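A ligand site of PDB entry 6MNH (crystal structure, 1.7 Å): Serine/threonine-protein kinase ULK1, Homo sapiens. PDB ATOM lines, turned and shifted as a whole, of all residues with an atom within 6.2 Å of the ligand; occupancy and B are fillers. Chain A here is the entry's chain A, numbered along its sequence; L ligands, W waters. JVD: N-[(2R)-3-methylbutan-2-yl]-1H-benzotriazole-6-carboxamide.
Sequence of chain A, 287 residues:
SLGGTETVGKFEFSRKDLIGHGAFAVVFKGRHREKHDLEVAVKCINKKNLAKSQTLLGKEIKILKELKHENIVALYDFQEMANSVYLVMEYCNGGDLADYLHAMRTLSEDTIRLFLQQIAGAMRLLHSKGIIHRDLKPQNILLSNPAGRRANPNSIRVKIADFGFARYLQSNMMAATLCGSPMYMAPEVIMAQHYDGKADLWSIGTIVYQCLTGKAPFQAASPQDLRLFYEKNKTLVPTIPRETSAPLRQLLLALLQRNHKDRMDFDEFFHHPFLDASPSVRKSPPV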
ATOM      1  N   ILE A  19     -15.454 -33.866 -14.089  1.00  0.00           N
ATOM      2  CA  ILE A  19     -16.733 -34.523 -13.833  1.00  0.00           C
ATOM      3  C   ILE A  19     -17.902 -33.874 -14.590  1.00  0.00           C
ATOM      4  O   ILE A  19     -19.015 -34.410 -14.584  1.00  0.00           O
ATOM      5  CB  ILE A  19     -17.037 -34.653 -12.322  1.00  0.00           C
ATOM      6  CG1 ILE A  19     -17.186 -33.294 -11.613  1.00  0.00           C
ATOM      7  CG2 ILE A  19     -16.007 -35.559 -11.641  1.00  0.00           C
ATOM      8  CD1 ILE A  19     -17.775 -33.352 -10.214  1.00  0.00           C
ATOM      9  N   GLY A  20     -17.681 -32.712 -15.196  1.00  0.00           N
ATOM     10  CA  GLY A  20     -18.732 -32.056 -15.963  1.00  0.00           C
ATOM     11  C   GLY A  20     -18.166 -31.047 -16.952  1.00  0.00           C
ATOM     12  O   GLY A  20     -17.162 -30.398 -16.683  1.00  0.00           O
ATOM     13  N   HIS A  21     -18.828 -30.919 -18.106  1.00  0.00           N
ATOM     14  CA  HIS A  21     -18.313 -30.060 -19.153  1.00  0.00           C
ATOM     15  C   HIS A  21     -19.467 -29.596 -20.034  1.00  0.00           C
ATOM     16  O   HIS A  21     -20.169 -30.417 -20.621  1.00  0.00           O
ATOM     17  CB  HIS A  21     -17.183 -30.784 -19.923  1.00  0.00           C
ATOM     18  CG  HIS A  21     -16.432 -29.934 -20.879  1.00  0.00           C
ATOM     19  ND1 HIS A  21     -15.554 -30.492 -21.799  1.00  0.00           N
ATOM     20  CD2 HIS A  21     -16.410 -28.599 -21.083  1.00  0.00           C
ATOM     21  CE1 HIS A  21     -15.031 -29.531 -22.539  1.00  0.00           C
ATOM     22  NE2 HIS A  21     -15.531 -28.358 -22.104  1.00  0.00           N
ATOM     23  N   GLY A  22     -19.696 -28.295 -20.017  1.00  0.00           N
ATOM     24  CA  GLY A  22     -20.705 -27.679 -20.866  1.00  0.00           C
ATOM     25  C   GLY A  22     -20.052 -26.539 -21.631  1.00  0.00           C
ATOM     26  O   GLY A  22     -18.854 -26.284 -21.446  1.00  0.00           O
ATOM     27  N   ALA A  23     -20.838 -25.866 -22.479  1.00  0.00           N
ATOM     28  CA  ALA A  23     -20.350 -24.732 -23.240  1.00  0.00           C
ATOM     29  C   ALA A  23     -19.874 -23.624 -22.300  1.00  0.00           C
ATOM     30  O   ALA A  23     -18.970 -22.869 -22.654  1.00  0.00           O
ATOM     31  CB  ALA A  23     -21.439 -24.229 -24.170  1.00  0.00           C
ATOM     32  N   PHE A  24     -20.473 -23.536 -21.104  1.00  0.00           N
ATOM     33  CA  PHE A  24     -20.265 -22.365 -20.245  1.00  0.00           C
ATOM     34  C   PHE A  24     -19.646 -22.696 -18.883  1.00  0.00           C
ATOM     35  O   PHE A  24     -19.541 -21.812 -18.038  1.00  0.00           O
ATOM     36  CB  PHE A  24     -21.548 -21.538 -20.130  1.00  0.00           C
ATOM     37  CG  PHE A  24     -22.152 -21.225 -21.472  1.00  0.00           C
ATOM     38  CD1 PHE A  24     -21.460 -20.459 -22.407  1.00  0.00           C
ATOM     39  CD2 PHE A  24     -23.395 -21.743 -21.831  1.00  0.00           C
ATOM     40  CE1 PHE A  24     -22.008 -20.198 -23.656  1.00  0.00           C
ATOM     41  CE2 PHE A  24     -23.948 -21.475 -23.074  1.00  0.00           C
ATOM     42  CZ  PHE A  24     -23.248 -20.705 -23.987  1.00  0.00           C
ATOM     43  N   ALA A  25     -19.219 -23.946 -18.687  1.00  0.00           N
ATOM     44  CA  ALA A  25     -18.567 -24.307 -17.431  1.00  0.00           C
ATOM     45  C   ALA A  25     -17.821 -25.635 -17.571  1.00  0.00           C
ATOM     46  O   ALA A  25     -18.200 -26.503 -18.352  1.00  0.00           O
ATOM     47  CB  ALA A  25     -19.574 -24.379 -16.298  1.00  0.00           C
ATOM     48  N   VAL A  26     -16.740 -25.756 -16.796  1.00  0.00           N
ATOM     49  CA  VAL A  26     -16.070 -27.034 -16.617  1.00  0.00           C
ATOM     50  C   VAL A  26     -16.087 -27.344 -15.121  1.00  0.00           C
ATOM     51  O   VAL A  26     -15.873 -26.444 -14.312  1.00  0.00           O
ATOM     52  CB  VAL A  26     -14.636 -27.016 -17.214  1.00  0.00           C
ATOM     53  CG1 VAL A  26     -14.066 -28.414 -17.331  1.00  0.00           C
ATOM     54  CG2 VAL A  26     -14.587 -26.371 -18.592  1.00  0.00           C
ATOM     55  N   VAL A  27     -16.374 -28.608 -14.761  1.00  0.00           N
ATOM     56  CA  VAL A  27     -16.581 -28.984 -13.365  1.00  0.00           C
ATOM     57  C   VAL A  27     -15.613 -30.084 -12.976  1.00  0.00           C
ATOM     58  O   VAL A  27     -15.508 -31.100 -13.656  1.00  0.00           O
ATOM     59  CB  VAL A  27     -18.043 -29.393 -13.065  1.00  0.00           C
ATOM     60  CG1 VAL A  27     -18.286 -29.488 -11.563  1.00  0.00           C
ATOM     61  CG2 VAL A  27     -19.063 -28.472 -13.695  1.00  0.00           C
ATOM     62  N   VAL A  40     -16.157 -32.120  -2.829  1.00  0.00           N
ATOM     63  CA  VAL A  40     -16.910 -31.034  -3.446  1.00  0.00           C
ATOM     64  C   VAL A  40     -16.778 -31.135  -4.961  1.00  0.00           C
ATOM     65  O   VAL A  40     -15.986 -31.915  -5.485  1.00  0.00           O
ATOM     66  CB  VAL A  40     -16.467 -29.632  -2.948  1.00  0.00           C
ATOM     67  CG1 VAL A  40     -16.768 -29.371  -1.472  1.00  0.00           C
ATOM     68  CG2 VAL A  40     -15.008 -29.328  -3.282  1.00  0.00           C
ATOM     69  N   ALA A  41     -17.587 -30.309  -5.646  1.00  0.00           N
ATOM     70  CA  ALA A  41     -17.448 -30.046  -7.071  1.00  0.00           C
ATOM     71  C   ALA A  41     -17.056 -28.573  -7.240  1.00  0.00           C
ATOM     72  O   ALA A  41     -17.615 -27.710  -6.577  1.00  0.00           O
ATOM     73  CB  ALA A  41     -18.757 -30.336  -7.789  1.00  0.00           C
ATOM     74  N   LYS A  43     -16.942 -25.706  -9.967  1.00  0.00           N
ATOM     75  CA  LYS A  43     -17.393 -25.239 -11.274  1.00  0.00           C
ATOM     76  C   LYS A  43     -16.582 -24.018 -11.708  1.00  0.00           C
ATOM     77  O   LYS A  43     -16.547 -23.008 -10.996  1.00  0.00           O
ATOM     78  CB  LYS A  43     -18.894 -24.926 -11.188  1.00  0.00           C
ATOM     79  CG  LYS A  43     -19.598 -24.702 -12.521  1.00  0.00           C
ATOM     80  CD  LYS A  43     -21.100 -24.673 -12.350  1.00  0.00           C
ATOM     81  CE  LYS A  43     -21.875 -24.634 -13.651  1.00  0.00           C
ATOM     82  NZ  LYS A  43     -23.330 -24.683 -13.400  1.00  0.00           N
ATOM     83  N   GLU A  60     -25.375 -17.316 -11.576  1.00  0.00           N
ATOM     84  CA  GLU A  60     -25.606 -18.532 -10.819  1.00  0.00           C
ATOM     85  C   GLU A  60     -25.254 -18.324  -9.350  1.00  0.00           C
ATOM     86  O   GLU A  60     -26.003 -18.775  -8.482  1.00  0.00           O
ATOM     87  CB  GLU A  60     -24.841 -19.719 -11.411  1.00  0.00           C
ATOM     88  CG  GLU A  60     -25.174 -21.045 -10.741  1.00  0.00           C
ATOM     89  CD  GLU A  60     -24.795 -22.302 -11.506  1.00  0.00           C
ATOM     90  OE1 GLU A  60     -23.810 -22.281 -12.261  1.00  0.00           O
ATOM     91  OE2 GLU A  60     -25.501 -23.312 -11.333  1.00  0.00           O
ATOM     92  N   VAL A  73     -28.684 -28.435  -5.959  1.00  0.00           N
ATOM     93  CA  VAL A  73     -27.256 -28.471  -5.625  1.00  0.00           C
ATOM     94  C   VAL A  73     -26.907 -27.272  -4.744  1.00  0.00           C
ATOM     95  O   VAL A  73     -27.214 -26.126  -5.094  1.00  0.00           O
ATOM     96  CB  VAL A  73     -26.373 -28.553  -6.887  1.00  0.00           C
ATOM     97  CG1 VAL A  73     -26.494 -27.317  -7.768  1.00  0.00           C
ATOM     98  CG2 VAL A  73     -24.911 -28.820  -6.549  1.00  0.00           C
ATOM     99  N   MET A  89     -19.296 -26.376  -4.853  1.00  0.00           N
ATOM    100  CA  MET A  89     -20.644 -26.906  -4.729  1.00  0.00           C
ATOM    101  C   MET A  89     -20.629 -28.341  -4.198  1.00  0.00           C
ATOM    102  O   MET A  89     -19.617 -29.049  -4.233  1.00  0.00           O
ATOM    103  CB  MET A  89     -21.358 -26.896  -6.090  1.00  0.00           C
ATOM    104  CG  MET A  89     -20.914 -25.766  -7.014  1.00  0.00           C
ATOM    105  SD  MET A  89     -21.970 -25.521  -8.454  1.00  0.00           S
ATOM    106  CE  MET A  89     -23.516 -25.148  -7.643  1.00  0.00           C
ATOM    107  N   GLU A  90     -21.805 -28.736  -3.727  1.00  0.00           N
ATOM    108  CA  GLU A  90     -22.149 -30.101  -3.361  1.00  0.00           C
ATOM    109  C   GLU A  90     -21.721 -31.035  -4.483  1.00  0.00           C
ATOM    110  O   GLU A  90     -21.991 -30.758  -5.653  1.00  0.00           O
ATOM    111  CB  GLU A  90     -23.663 -30.108  -3.127  1.00  0.00           C
ATOM    112  CG  GLU A  90     -24.259 -31.491  -2.891  1.00  0.00           C
ATOM    113  CD  GLU A  90     -25.726 -31.452  -2.493  1.00  0.00           C
ATOM    114  OE1 GLU A  90     -26.174 -32.416  -1.857  1.00  0.00           O
ATOM    115  OE2 GLU A  90     -26.404 -30.458  -2.819  1.00  0.00           O
ATOM    116  N   TYR A  91     -20.989 -32.095  -4.108  1.00  0.00           N
ATOM    117  CA  TYR A  91     -20.597 -33.160  -5.017  1.00  0.00           C
ATOM    118  C   TYR A  91     -21.741 -34.161  -5.142  1.00  0.00           C
ATOM    119  O   TYR A  91     -22.277 -34.632  -4.129  1.00  0.00           O
ATOM    120  CB  TYR A  91     -19.303 -33.851  -4.561  1.00  0.00           C
ATOM    121  CG  TYR A  91     -18.874 -35.050  -5.377  1.00  0.00           C
ATOM    122  CD1 TYR A  91     -18.647 -34.957  -6.751  1.00  0.00           C
ATOM    123  CD2 TYR A  91     -18.695 -36.284  -4.787  1.00  0.00           C
ATOM    124  CE1 TYR A  91     -18.264 -36.053  -7.500  1.00  0.00           C
ATOM    125  CE2 TYR A  91     -18.298 -37.398  -5.515  1.00  0.00           C
ATOM    126  CZ  TYR A  91     -18.083 -37.277  -6.881  1.00  0.00           C
ATOM    127  OH  TYR A  91     -17.692 -38.369  -7.606  1.00  0.00           O
ATOM    128  N   CYS A  92     -22.121 -34.439  -6.394  1.00  0.00           N
ATOM    129  CA  CYS A  92     -23.124 -35.448  -6.731  1.00  0.00           C
ATOM    130  C   CYS A  92     -22.389 -36.593  -7.416  1.00  0.00           C
ATOM    131  O   CYS A  92     -21.822 -36.428  -8.503  1.00  0.00           O
ATOM    132  CB  CYS A  92     -24.207 -34.832  -7.617  1.00  0.00           C
ATOM    133  SG  CYS A  92     -25.115 -33.462  -6.845  1.00  0.00           S
ATOM    134  N   ASN A  93     -22.350 -37.764  -6.754  1.00  0.00           N
ATOM    135  CA  ASN A  93     -21.417 -38.822  -7.114  1.00  0.00           C
ATOM    136  C   ASN A  93     -22.008 -39.797  -8.141  1.00  0.00           C
ATOM    137  O   ASN A  93     -21.355 -40.788  -8.479  1.00  0.00           O
ATOM    138  CB  ASN A  93     -20.985 -39.623  -5.873  1.00  0.00           C
ATOM    139  CG  ASN A  93     -22.130 -40.252  -5.112  1.00  0.00           C
ATOM    140  OD1 ASN A  93     -23.221 -40.450  -5.658  1.00  0.00           O
ATOM    141  ND2 ASN A  93     -21.906 -40.590  -3.860  1.00  0.00           N
ATOM    142  N   ASP A  96     -25.145 -37.680 -14.178  1.00  0.00           N
ATOM    143  CA  ASP A  96     -26.358 -36.914 -14.456  1.00  0.00           C
ATOM    144  C   ASP A  96     -27.397 -37.835 -15.101  1.00  0.00           C
ATOM    145  O   ASP A  96     -27.122 -38.990 -15.384  1.00  0.00           O
ATOM    146  CB  ASP A  96     -26.060 -35.677 -15.295  1.00  0.00           C
ATOM    147  CG  ASP A  96     -25.353 -35.989 -16.608  1.00  0.00           C
ATOM    148  OD1 ASP A  96     -25.835 -36.858 -17.350  1.00  0.00           O
ATOM    149  OD2 ASP A  96     -24.287 -35.416 -16.858  1.00  0.00           O
ATOM    150  N   LYS A 137     -32.826 -29.863 -18.551  1.00  0.00           N
ATOM    151  CA  LYS A 137     -32.483 -30.903 -19.504  1.00  0.00           C
ATOM    152  C   LYS A 137     -31.784 -32.021 -18.733  1.00  0.00           C
ATOM    153  O   LYS A 137     -31.367 -31.802 -17.601  1.00  0.00           O
ATOM    154  CB  LYS A 137     -31.583 -30.348 -20.614  1.00  0.00           C
ATOM    155  CG  LYS A 137     -30.247 -29.789 -20.137  1.00  0.00           C
ATOM    156  CD  LYS A 137     -29.598 -28.879 -21.142  1.00  0.00           C
ATOM    157  CE  LYS A 137     -28.334 -28.264 -20.597  1.00  0.00           C
ATOM    158  NZ  LYS A 137     -28.021 -26.985 -21.279  1.00  0.00           N
ATOM    159  N   GLN A 139     -28.876 -33.229 -18.686  1.00  0.00           N
ATOM    160  CA  GLN A 139     -27.508 -32.889 -18.328  1.00  0.00           C
ATOM    161  C   GLN A 139     -27.425 -32.083 -17.027  1.00  0.00           C
ATOM    162  O   GLN A 139     -26.373 -32.073 -16.390  1.00  0.00           O
ATOM    163  CB  GLN A 139     -26.820 -32.088 -19.442  1.00  0.00           C
ATOM    164  CG  GLN A 139     -26.512 -32.889 -20.697  1.00  0.00           C
ATOM    165  CD  GLN A 139     -27.707 -33.169 -21.577  1.00  0.00           C
ATOM    166  OE1 GLN A 139     -28.750 -32.511 -21.502  1.00  0.00           O
ATOM    167  NE2 GLN A 139     -27.572 -34.161 -22.446  1.00  0.00           N
ATOM    168  N   ASN A 140     -28.517 -31.402 -16.647  1.00  0.00           N
ATOM    169  CA  ASN A 140     -28.433 -30.638 -15.404  1.00  0.00           C
ATOM    170  C   ASN A 140     -29.393 -31.178 -14.337  1.00  0.00           C
ATOM    171  O   ASN A 140     -29.673 -30.499 -13.346  1.00  0.00           O
ATOM    172  CB  ASN A 140     -28.417 -29.121 -15.636  1.00  0.00           C
ATOM    173  CG  ASN A 140     -29.583 -28.597 -16.431  1.00  0.00           C
ATOM    174  OD1 ASN A 140     -30.687 -29.138 -16.349  1.00  0.00           O
ATOM    175  ND2 ASN A 140     -29.348 -27.515 -17.172  1.00  0.00           N
ATOM    176  N   LEU A 142     -28.847 -33.801 -11.716  1.00  0.00           N
ATOM    177  CA  LEU A 142     -27.721 -34.555 -11.180  1.00  0.00           C
ATOM    178  C   LEU A 142     -28.203 -35.644 -10.232  1.00  0.00           C
ATOM    179  O   LEU A 142     -29.189 -35.434  -9.528  1.00  0.00           O
ATOM    180  CB  LEU A 142     -26.795 -33.591 -10.425  1.00  0.00           C
ATOM    181  CG  LEU A 142     -26.267 -32.382 -11.194  1.00  0.00           C
ATOM    182  CD1 LEU A 142     -25.241 -31.644 -10.336  1.00  0.00           C
ATOM    183  CD2 LEU A 142     -25.643 -32.785 -12.521  1.00  0.00           C
ATOM    184  N   ALA A 161     -29.260 -28.674 -11.085  1.00  0.00           N
ATOM    185  CA  ALA A 161     -28.071 -27.835 -11.167  1.00  0.00           C
ATOM    186  C   ALA A 161     -28.242 -26.791 -12.270  1.00  0.00           C
ATOM    187  O   ALA A 161     -29.275 -26.760 -12.946  1.00  0.00           O
ATOM    188  CB  ALA A 161     -26.870 -28.697 -11.436  1.00  0.00           C
ATOM    189  N   ASP A 162     -27.231 -25.908 -12.394  1.00  0.00           N
ATOM    190  CA  ASP A 162     -26.961 -25.128 -13.599  1.00  0.00           C
ATOM    191  C   ASP A 162     -27.970 -23.991 -13.696  1.00  0.00           C
ATOM    192  O   ASP A 162     -28.812 -23.978 -14.600  1.00  0.00           O
ATOM    193  CB  ASP A 162     -26.909 -26.045 -14.827  1.00  0.00           C
ATOM    194  CG  ASP A 162     -26.022 -25.580 -15.962  1.00  0.00           C
ATOM    195  OD1 ASP A 162     -25.070 -24.817 -15.706  1.00  0.00           O
ATOM    196  OD2 ASP A 162     -26.277 -26.037 -17.109  1.00  0.00           O
HETATM  197  C1  JVD L   1     -22.844 -28.606 -10.602  1.00  0.00           C
HETATM  198  C2  JVD L   1     -22.583 -29.166  -9.334  1.00  0.00           C
HETATM  199  C3  JVD L   1     -22.193 -30.671 -11.749  1.00  0.00           C
HETATM  200  C4  JVD L   1     -22.651 -29.341 -11.785  1.00  0.00           C
HETATM  201  C5  JVD L   1     -21.948 -31.196 -10.468  1.00  0.00           C
HETATM  202  C6  JVD L   1     -22.125 -30.494  -9.280  1.00  0.00           C
HETATM  203  C7  JVD L   1     -22.989 -28.631 -13.043  1.00  0.00           C
HETATM  204  C8  JVD L   1     -21.235 -29.412 -16.744  1.00  0.00           C
HETATM  205  C9  JVD L   1     -22.467 -27.381 -17.532  1.00  0.00           C
HETATM  206  C10 JVD L   1     -24.402 -29.301 -16.154  1.00  0.00           C
HETATM  207  C11 JVD L   1     -22.052 -28.208 -16.312  1.00  0.00           C
HETATM  208  C12 JVD L   1     -23.286 -28.567 -15.422  1.00  0.00           C
HETATM  209  N13 JVD L   1     -21.512 -32.423 -10.031  1.00  0.00           N
HETATM  210  N14 JVD L   1     -21.419 -32.471  -8.681  1.00  0.00           N
HETATM  211  N15 JVD L   1     -21.817 -31.286  -8.199  1.00  0.00           N
HETATM  212  N16 JVD L   1     -22.904 -29.330 -14.227  1.00  0.00           N
HETATM  213  O17 JVD L   1     -23.378 -27.454 -12.991  1.00  0.00           O
HETATM  214  O   HOH W   1     -22.561 -24.946 -19.927  1.00  0.00           O
HETATM  215  O   HOH W   2     -22.919 -24.520 -17.198  1.00  0.00           O
HETATM  216  O   HOH W   3     -22.035 -32.101 -14.612  1.00  0.00           O
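N15 of the ligand sits close to O of Glu 90.
NZ of Lys 43 is in hydrogen-bond range of O17 of the ligand (2.8 Å).
The backbone NH (N) of Cys 92 lies within hydrogen-bond range of a nitrogen (N14) of the ligand (3.1 Å).
The side-chain amino group (NZ) of Lys 43 is in salt-bridge range of the side-chain carboxylate (OD1) of Asp 162.
The side-chain amino group of Lys 43 lies within salt-bridge range of the side-chain carboxylate of Glu 60 (2.7 Å).
The backbone carbonyl oxygen of Ala 41 sits at hydrogen-bond distance from the backbone NH of Met 89 (2.8 Å).
O of Gly 20 lies within hydrogen-bond range of N of Val 27, 2.7 Å away.
The backbone NH (N) of Ile 19 lies within hydrogen-bond range of the backbone carbonyl oxygen (O) of Val 27 (2.8 Å).
The side-chain amide nitrogen (ND2) of Asn 140 is in hydrogen-bond range of the side-chain carboxylate (OD2) of Asp 162.
N of Asp 162 lies close to OE2 of Glu 60, at 3.3 Å.
Residues that only touch the ligand: His 21 (3.1 Å), Ala 41 (3.2 Å), Leu 142 (3.3 Å), Gln 139 (3.4 Å), Gly 20 (3.5 Å), Val 73 (3.6 Å), Gly 22 (3.8 Å), Met 89 (3.8 Å), Tyr 91 (3.8 Å), Ile 19 (3.9 Å), Val 27 (3.9 Å) and Asp 162 (3.9 Å).
15 residues have an atom within 4 Å of the ligand: Ile 19, Gly 20, His 21, Gly 22, Val 27, Ala 41, Lys 43, Val 73, Met 89, Glu 90, Tyr 91, Cys 92, Gln 139, Leu 142 and Asp 162.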
